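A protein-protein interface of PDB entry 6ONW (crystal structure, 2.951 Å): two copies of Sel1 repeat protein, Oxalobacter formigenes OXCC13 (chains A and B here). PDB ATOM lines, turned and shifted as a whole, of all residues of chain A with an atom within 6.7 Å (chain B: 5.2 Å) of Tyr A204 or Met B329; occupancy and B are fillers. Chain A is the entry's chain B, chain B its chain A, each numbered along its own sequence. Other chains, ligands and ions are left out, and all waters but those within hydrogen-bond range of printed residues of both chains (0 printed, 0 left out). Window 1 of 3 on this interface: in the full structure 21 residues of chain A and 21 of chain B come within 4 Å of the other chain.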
ATOM      1  N   ASN A  24     -12.618   7.358 -21.446  1.00  0.00           N
ATOM      2  CA  ASN A  24     -12.407   6.515 -22.617  1.00  0.00           C
ATOM      3  C   ASN A  24     -13.610   5.647 -22.954  1.00  0.00           C
ATOM      4  O   ASN A  24     -13.566   4.920 -23.952  1.00  0.00           O
ATOM      5  CB  ASN A  24     -11.178   5.623 -22.412  1.00  0.00           C
ATOM      6  CG  ASN A  24      -9.882   6.316 -22.790  1.00  0.00           C
ATOM      7  OD1 ASN A  24      -9.865   7.202 -23.645  1.00  0.00           O
ATOM      8  ND2 ASN A  24      -8.786   5.905 -22.162  1.00  0.00           N
ATOM      9  N   GLU A  25     -14.676   5.704 -22.161  1.00  0.00           N
ATOM     10  CA  GLU A  25     -15.843   4.859 -22.370  1.00  0.00           C
ATOM     11  C   GLU A  25     -16.789   5.486 -23.387  1.00  0.00           C
ATOM     12  O   GLU A  25     -16.856   6.709 -23.536  1.00  0.00           O
ATOM     13  CB  GLU A  25     -16.575   4.619 -21.047  1.00  0.00           C
ATOM     14  CG  GLU A  25     -17.572   3.469 -21.087  1.00  0.00           C
ATOM     15  CD  GLU A  25     -18.219   3.204 -19.742  1.00  0.00           C
ATOM     16  OE1 GLU A  25     -17.867   3.897 -18.763  1.00  0.00           O
ATOM     17  OE2 GLU A  25     -19.081   2.302 -19.665  1.00  0.00           O
ATOM     18  N   GLU A  26     -17.518   4.626 -24.092  1.00  0.00           N
ATOM     19  CA  GLU A  26     -18.480   5.086 -25.084  1.00  0.00           C
ATOM     20  C   GLU A  26     -19.565   5.924 -24.415  1.00  0.00           C
ATOM     21  O   GLU A  26     -20.141   5.494 -23.406  1.00  0.00           O
ATOM     22  CB  GLU A  26     -19.103   3.889 -25.804  1.00  0.00           C
ATOM     23  CG  GLU A  26     -20.330   4.223 -26.635  1.00  0.00           C
ATOM     24  CD  GLU A  26     -20.009   5.076 -27.845  1.00  0.00           C
ATOM     25  OE1 GLU A  26     -18.868   4.999 -28.348  1.00  0.00           O
ATOM     26  OE2 GLU A  26     -20.900   5.830 -28.289  1.00  0.00           O
ATOM     27  N   LEU A  28     -22.578   6.425 -25.214  1.00  0.00           N
ATOM     28  CA  LEU A  28     -23.874   5.757 -25.212  1.00  0.00           C
ATOM     29  C   LEU A  28     -24.042   4.894 -23.968  1.00  0.00           C
ATOM     30  O   LEU A  28     -25.086   4.932 -23.306  1.00  0.00           O
ATOM     31  CB  LEU A  28     -24.030   4.917 -26.481  1.00  0.00           C
ATOM     32  CG  LEU A  28     -25.306   4.082 -26.599  1.00  0.00           C
ATOM     33  CD1 LEU A  28     -26.541   4.957 -26.440  1.00  0.00           C
ATOM     34  CD2 LEU A  28     -25.332   3.349 -27.931  1.00  0.00           C
ATOM     35  N   PHE A  29     -23.015   4.113 -23.629  1.00  0.00           N
ATOM     36  CA  PHE A  29     -23.100   3.253 -22.455  1.00  0.00           C
ATOM     37  C   PHE A  29     -23.045   4.059 -21.163  1.00  0.00           C
ATOM     38  O   PHE A  29     -23.574   3.617 -20.138  1.00  0.00           O
ATOM     39  CB  PHE A  29     -21.980   2.212 -22.487  1.00  0.00           C
ATOM     40  CG  PHE A  29     -22.004   1.334 -23.708  1.00  0.00           C
ATOM     41  CD1 PHE A  29     -23.204   0.995 -24.311  1.00  0.00           C
ATOM     42  CD2 PHE A  29     -20.825   0.854 -24.255  1.00  0.00           C
ATOM     43  CE1 PHE A  29     -23.230   0.190 -25.437  1.00  0.00           C
ATOM     44  CE2 PHE A  29     -20.843   0.048 -25.381  1.00  0.00           C
ATOM     45  CZ  PHE A  29     -22.047  -0.283 -25.972  1.00  0.00           C
ATOM     46  N   GLY A 164     -30.572   3.473 -29.322  1.00  0.00           N
ATOM     47  CA  GLY A 164     -29.152   3.289 -29.551  1.00  0.00           C
ATOM     48  C   GLY A 164     -28.603   2.008 -28.964  1.00  0.00           C
ATOM     49  O   GLY A 164     -27.611   1.470 -29.466  1.00  0.00           O
ATOM     50  N   ARG A 171     -32.678  -1.556 -32.978  1.00  0.00           N
ATOM     51  CA  ARG A 171     -31.672  -0.503 -32.993  1.00  0.00           C
ATOM     52  C   ARG A 171     -31.879   0.410 -34.196  1.00  0.00           C
ATOM     53  O   ARG A 171     -32.011  -0.058 -35.331  1.00  0.00           O
ATOM     54  CB  ARG A 171     -30.266  -1.100 -33.019  1.00  0.00           C
ATOM     55  CG  ARG A 171     -29.184  -0.077 -33.345  1.00  0.00           C
ATOM     56  CD  ARG A 171     -27.783  -0.671 -33.299  1.00  0.00           C
ATOM     57  NE  ARG A 171     -27.315  -0.879 -31.932  1.00  0.00           N
ATOM     58  CZ  ARG A 171     -26.047  -1.109 -31.608  1.00  0.00           C
ATOM     59  NH1 ARG A 171     -25.116  -1.154 -32.553  1.00  0.00           N
ATOM     60  NH2 ARG A 171     -25.705  -1.287 -30.338  1.00  0.00           N
ATOM     61  N   LEU A 173     -30.182   4.253 -34.983  1.00  0.00           N
ATOM     62  CA  LEU A 173     -29.439   5.421 -34.521  1.00  0.00           C
ATOM     63  C   LEU A 173     -30.121   6.722 -34.923  1.00  0.00           C
ATOM     64  O   LEU A 173     -30.018   7.721 -34.201  1.00  0.00           O
ATOM     65  CB  LEU A 173     -28.008   5.376 -35.058  1.00  0.00           C
ATOM     66  CG  LEU A 173     -26.937   4.811 -34.118  1.00  0.00           C
ATOM     67  CD1 LEU A 173     -27.380   3.500 -33.486  1.00  0.00           C
ATOM     68  CD2 LEU A 173     -25.628   4.624 -34.865  1.00  0.00           C
ATOM     69  N   PHE A 198     -22.686  12.615 -27.855  1.00  0.00           N
ATOM     70  CA  PHE A 198     -22.855  11.757 -29.023  1.00  0.00           C
ATOM     71  C   PHE A 198     -22.268  12.375 -30.284  1.00  0.00           C
ATOM     72  O   PHE A 198     -21.909  11.641 -31.211  1.00  0.00           O
ATOM     73  CB  PHE A 198     -24.337  11.445 -29.247  1.00  0.00           C
ATOM     74  CG  PHE A 198     -24.951  10.586 -28.177  1.00  0.00           C
ATOM     75  CD1 PHE A 198     -24.156   9.906 -27.268  1.00  0.00           C
ATOM     76  CD2 PHE A 198     -26.326  10.455 -28.085  1.00  0.00           C
ATOM     77  CE1 PHE A 198     -24.723   9.118 -26.285  1.00  0.00           C
ATOM     78  CE2 PHE A 198     -26.899   9.667 -27.105  1.00  0.00           C
ATOM     79  CZ  PHE A 198     -26.097   8.997 -26.205  1.00  0.00           C
ATOM     80  N   SER A 202     -18.509   9.788 -29.486  1.00  0.00           N
ATOM     81  CA  SER A 202     -19.134   8.499 -29.734  1.00  0.00           C
ATOM     82  C   SER A 202     -18.630   7.898 -31.039  1.00  0.00           C
ATOM     83  O   SER A 202     -18.292   8.612 -31.986  1.00  0.00           O
ATOM     84  CB  SER A 202     -20.657   8.631 -29.782  1.00  0.00           C
ATOM     85  OG  SER A 202     -21.261   7.385 -30.086  1.00  0.00           O
ATOM     86  N   HIS A 203     -18.579   6.567 -31.075  1.00  0.00           N
ATOM     87  CA  HIS A 203     -18.275   5.836 -32.295  1.00  0.00           C
ATOM     88  C   HIS A 203     -19.516   5.248 -32.951  1.00  0.00           C
ATOM     89  O   HIS A 203     -19.444   4.829 -34.111  1.00  0.00           O
ATOM     90  CB  HIS A 203     -17.259   4.723 -32.012  1.00  0.00           C
ATOM     91  CG  HIS A 203     -15.916   5.230 -31.584  1.00  0.00           C
ATOM     92  ND1 HIS A 203     -15.034   5.827 -32.459  1.00  0.00           N
ATOM     93  CD2 HIS A 203     -15.306   5.231 -30.376  1.00  0.00           C
ATOM     94  CE1 HIS A 203     -13.939   6.174 -31.807  1.00  0.00           C
ATOM     95  NE2 HIS A 203     -14.078   5.823 -30.541  1.00  0.00           N
ATOM     96  N   TYR A 204     -20.643   5.204 -32.239  1.00  0.00           N
ATOM     97  CA  TYR A 204     -21.914   4.857 -32.864  1.00  0.00           C
ATOM     98  C   TYR A 204     -22.472   6.042 -33.646  1.00  0.00           C
ATOM     99  O   TYR A 204     -22.677   5.959 -34.862  1.00  0.00           O
ATOM    100  CB  TYR A 204     -22.922   4.398 -31.804  1.00  0.00           C
ATOM    101  CG  TYR A 204     -22.648   3.030 -31.211  1.00  0.00           C
ATOM    102  CD1 TYR A 204     -22.851   1.875 -31.954  1.00  0.00           C
ATOM    103  CD2 TYR A 204     -22.210   2.896 -29.899  1.00  0.00           C
ATOM    104  CE1 TYR A 204     -22.611   0.624 -31.415  1.00  0.00           C
ATOM    105  CE2 TYR A 204     -21.969   1.649 -29.349  1.00  0.00           C
ATOM    106  CZ  TYR A 204     -22.170   0.517 -30.112  1.00  0.00           C
ATOM    107  OH  TYR A 204     -21.931  -0.725 -29.570  1.00  0.00           O
ATOM    108  N   TYR A 205     -22.712   7.155 -32.962  1.00  0.00           N
ATOM    109  CA  TYR A 205     -23.275   8.342 -33.580  1.00  0.00           C
ATOM    110  C   TYR A 205     -22.208   9.105 -34.361  1.00  0.00           C
ATOM    111  O   TYR A 205     -21.014   8.984 -34.082  1.00  0.00           O
ATOM    112  CB  TYR A 205     -23.895   9.236 -32.509  1.00  0.00           C
ATOM    113  CG  TYR A 205     -24.959   8.543 -31.688  1.00  0.00           C
ATOM    114  CD1 TYR A 205     -26.240   8.359 -32.191  1.00  0.00           C
ATOM    115  CD2 TYR A 205     -24.682   8.071 -30.412  1.00  0.00           C
ATOM    116  CE1 TYR A 205     -27.218   7.727 -31.446  1.00  0.00           C
ATOM    117  CE2 TYR A 205     -25.653   7.439 -29.658  1.00  0.00           C
ATOM    118  CZ  TYR A 205     -26.919   7.268 -30.181  1.00  0.00           C
ATOM    119  OH  TYR A 205     -27.887   6.638 -29.435  1.00  0.00           O
ATOM    120  N   PRO A 206     -22.615   9.894 -35.355  1.00  0.00           N
ATOM    121  CA  PRO A 206     -21.636  10.625 -36.169  1.00  0.00           C
ATOM    122  C   PRO A 206     -21.012  11.784 -35.403  1.00  0.00           C
ATOM    123  O   PRO A 206     -21.401  12.122 -34.282  1.00  0.00           O
ATOM    124  CB  PRO A 206     -22.463  11.121 -37.358  1.00  0.00           C
ATOM    125  CG  PRO A 206     -23.854  11.196 -36.836  1.00  0.00           C
ATOM    126  CD  PRO A 206     -23.987  10.057 -35.870  1.00  0.00           C
ATOM    127  N   PHE B 324     -11.161  -5.929 -35.095  1.00  0.00           N
ATOM    128  CA  PHE B 324     -10.473  -5.046 -34.160  1.00  0.00           C
ATOM    129  C   PHE B 324     -11.349  -3.860 -33.781  1.00  0.00           C
ATOM    130  O   PHE B 324     -11.371  -3.438 -32.620  1.00  0.00           O
ATOM    131  CB  PHE B 324      -9.159  -4.558 -34.768  1.00  0.00           C
ATOM    132  CG  PHE B 324      -8.097  -5.616 -34.859  1.00  0.00           C
ATOM    133  CD1 PHE B 324      -7.949  -6.562 -33.857  1.00  0.00           C
ATOM    134  CD2 PHE B 324      -7.243  -5.661 -35.947  1.00  0.00           C
ATOM    135  CE1 PHE B 324      -6.968  -7.531 -33.943  1.00  0.00           C
ATOM    136  CE2 PHE B 324      -6.262  -6.628 -36.039  1.00  0.00           C
ATOM    137  CZ  PHE B 324      -6.121  -7.563 -35.035  1.00  0.00           C
ATOM    138  N   TYR B 325     -12.085  -3.317 -34.753  1.00  0.00           N
ATOM    139  CA  TYR B 325     -12.931  -2.156 -34.498  1.00  0.00           C
ATOM    140  C   TYR B 325     -14.042  -2.483 -33.509  1.00  0.00           C
ATOM    141  O   TYR B 325     -14.329  -1.693 -32.602  1.00  0.00           O
ATOM    142  CB  TYR B 325     -13.511  -1.649 -35.820  1.00  0.00           C
ATOM    143  CG  TYR B 325     -14.522  -0.531 -35.692  1.00  0.00           C
ATOM    144  CD1 TYR B 325     -14.113   0.781 -35.483  1.00  0.00           C
ATOM    145  CD2 TYR B 325     -15.883  -0.781 -35.805  1.00  0.00           C
ATOM    146  CE1 TYR B 325     -15.032   1.808 -35.375  1.00  0.00           C
ATOM    147  CE2 TYR B 325     -16.809   0.237 -35.700  1.00  0.00           C
ATOM    148  CZ  TYR B 325     -16.378   1.531 -35.484  1.00  0.00           C
ATOM    149  OH  TYR B 325     -17.297   2.551 -35.378  1.00  0.00           O
ATOM    150  N   LYS B 326     -14.674  -3.649 -33.659  1.00  0.00           N
ATOM    151  CA  LYS B 326     -15.802  -3.991 -32.800  1.00  0.00           C
ATOM    152  C   LYS B 326     -15.366  -4.207 -31.356  1.00  0.00           C
ATOM    153  O   LYS B 326     -16.163  -4.004 -30.433  1.00  0.00           O
ATOM    154  CB  LYS B 326     -16.513  -5.232 -33.340  1.00  0.00           C
ATOM    155  CG  LYS B 326     -18.007  -5.261 -33.063  1.00  0.00           C
ATOM    156  CD  LYS B 326     -18.705  -6.303 -33.922  1.00  0.00           C
ATOM    157  CE  LYS B 326     -20.216  -6.231 -33.763  1.00  0.00           C
ATOM    158  NZ  LYS B 326     -20.913  -7.212 -34.639  1.00  0.00           N
ATOM    159  N   ALA B 327     -14.115  -4.612 -31.138  1.00  0.00           N
ATOM    160  CA  ALA B 327     -13.591  -4.760 -29.788  1.00  0.00           C
ATOM    161  C   ALA B 327     -12.929  -3.490 -29.276  1.00  0.00           C
ATOM    162  O   ALA B 327     -12.860  -3.282 -28.059  1.00  0.00           O
ATOM    163  CB  ALA B 327     -12.588  -5.915 -29.731  1.00  0.00           C
ATOM    164  N   ALA B 328     -12.442  -2.634 -30.179  1.00  0.00           N
ATOM    165  CA  ALA B 328     -11.809  -1.391 -29.752  1.00  0.00           C
ATOM    166  C   ALA B 328     -12.811  -0.440 -29.112  1.00  0.00           C
ATOM    167  O   ALA B 328     -12.447   0.322 -28.208  1.00  0.00           O
ATOM    168  CB  ALA B 328     -11.123  -0.717 -30.940  1.00  0.00           C
ATOM    169  N   MET B 329     -14.061  -0.466 -29.557  1.00  0.00           N
ATOM    170  CA  MET B 329     -15.092   0.395 -28.992  1.00  0.00           C
ATOM    171  C   MET B 329     -15.451  -0.037 -27.578  1.00  0.00           C
ATOM    172  O   MET B 329     -15.845   0.783 -26.749  1.00  0.00           O
ATOM    173  CB  MET B 329     -16.340   0.390 -29.873  1.00  0.00           C
ATOM    174  CG  MET B 329     -16.130   0.995 -31.245  1.00  0.00           C
ATOM    175  SD  MET B 329     -17.692   0.762 -32.378  1.00  0.00           S
ATOM    176  CE  MET B 329     -19.013   1.638 -31.247  1.00  0.00           C
ATOM    177  N   GLN B 330     -15.313  -1.333 -27.309  1.00  0.00           N
ATOM    178  CA  GLN B 330     -15.591  -1.868 -25.984  1.00  0.00           C
ATOM    179  C   GLN B 330     -14.421  -1.707 -25.022  1.00  0.00           C
ATOM    180  O   GLN B 330     -14.502  -2.195 -23.889  1.00  0.00           O
ATOM    181  CB  GLN B 330     -15.989  -3.343 -26.087  1.00  0.00           C
ATOM    182  CG  GLN B 330     -17.275  -3.571 -26.864  1.00  0.00           C
ATOM    183  CD  GLN B 330     -17.771  -5.000 -26.774  1.00  0.00           C
ATOM    184  OE1 GLN B 330     -16.993  -5.925 -26.544  1.00  0.00           O
ATOM    185  NE2 GLN B 330     -19.075  -5.187 -26.947  1.00  0.00           N
ATOM    186  N   GLY B 331     -13.347  -1.043 -25.438  1.00  0.00           N
ATOM    187  CA  GLY B 331     -12.250  -0.720 -24.550  1.00  0.00           C
ATOM    188  C   GLY B 331     -11.058  -1.648 -24.599  1.00  0.00           C
ATOM    189  O   GLY B 331     -10.174  -1.529 -23.743  1.00  0.00           O
ATOM    190  N   TRP B 359      -7.100   6.200 -32.027  1.00  0.00           N
ATOM    191  CA  TRP B 359      -7.099   4.930 -31.314  1.00  0.00           C
ATOM    192  C   TRP B 359      -5.787   4.679 -30.585  1.00  0.00           C
ATOM    193  O   TRP B 359      -5.771   3.950 -29.588  1.00  0.00           O
ATOM    194  CB  TRP B 359      -7.381   3.778 -32.279  1.00  0.00           C
ATOM    195  CG  TRP B 359      -8.772   3.771 -32.831  1.00  0.00           C
ATOM    196  CD1 TRP B 359      -9.149   4.074 -34.105  1.00  0.00           C
ATOM    197  CD2 TRP B 359      -9.974   3.441 -32.124  1.00  0.00           C
ATOM    198  NE1 TRP B 359     -10.511   3.954 -34.237  1.00  0.00           N
ATOM    199  CE2 TRP B 359     -11.041   3.567 -33.034  1.00  0.00           C
ATOM    200  CE3 TRP B 359     -10.250   3.053 -30.809  1.00  0.00           C
ATOM    201  CZ2 TRP B 359     -12.364   3.318 -32.674  1.00  0.00           C
ATOM    202  CZ3 TRP B 359     -11.564   2.806 -30.453  1.00  0.00           C
ATOM    203  CH2 TRP B 359     -12.604   2.939 -31.381  1.00  0.00           C
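O of His A203 lies within hydrogen-bond range of OH of Tyr B325 (3.4 Å).
The side-chain hydroxyl (OH) of Tyr B325 sits close to the side-chain sulfur (SD) of Met B329, at 3.5 Å. The side-chain hydroxyl (OG) of Ser A202 lies within hydrogen-bond range of the backbone NH (N) of Tyr A204 (3.1 Å). The backbone NH of His A203 lies within hydrogen-bond range of the side-chain carboxylate of Glu A26 (3.2 Å).
CB of His A203 touches CE of Met B329, at 3.6 Å. NE2 of His A203 touches CH2 of Trp B359, 3.3 Å away. Met B329 touches Tyr A204 (CE to CE2, 3.5 Å).
Arg A171 touches none of the printed residues of chain B. Printed residues of chain B within 4 Å of His A203: Tyr B325 (3.4 Å), Met B329 (3.6 Å) and Trp B359 (3.3 Å). Of chain B, only Met B329 comes within 4 Å of Tyr A204. Lys B326 touches none of the printed residues of chain A. Met B329 touches just these residues of chain A: His A203 and Tyr A204. Printed residues of chain A within 4 Å of Trp B359: His A203 (3.3 Å).
Of the 14 printed residues of chain A, 2 touch a printed residue of chain B. Hydrophobic or aromatic side chains of chain A within 4 Å of the printed part of chain B: His A203 and Tyr A204. Of the 9 printed residues of chain B, 3 touch a printed residue of chain A. Printed residues of chain B that touch a printed residue of chain A: Tyr B325, Met B329 and Trp B359. Hydrophobic or aromatic side chains of chain B that line the printed part of chain A: Tyr B325, Met B329 and Trp B359. Among the printed residues, 4 pairs touch across the chains. Among the printed residues, no Asp or Glu carboxylate lies within 4 Å of a Lys or Arg side-chain nitrogen of the other chain.
No position is printed for both chains. Of the 4 pairs that touch across the chains among the printed residues, none has its exchanged pair printed and touching as well.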
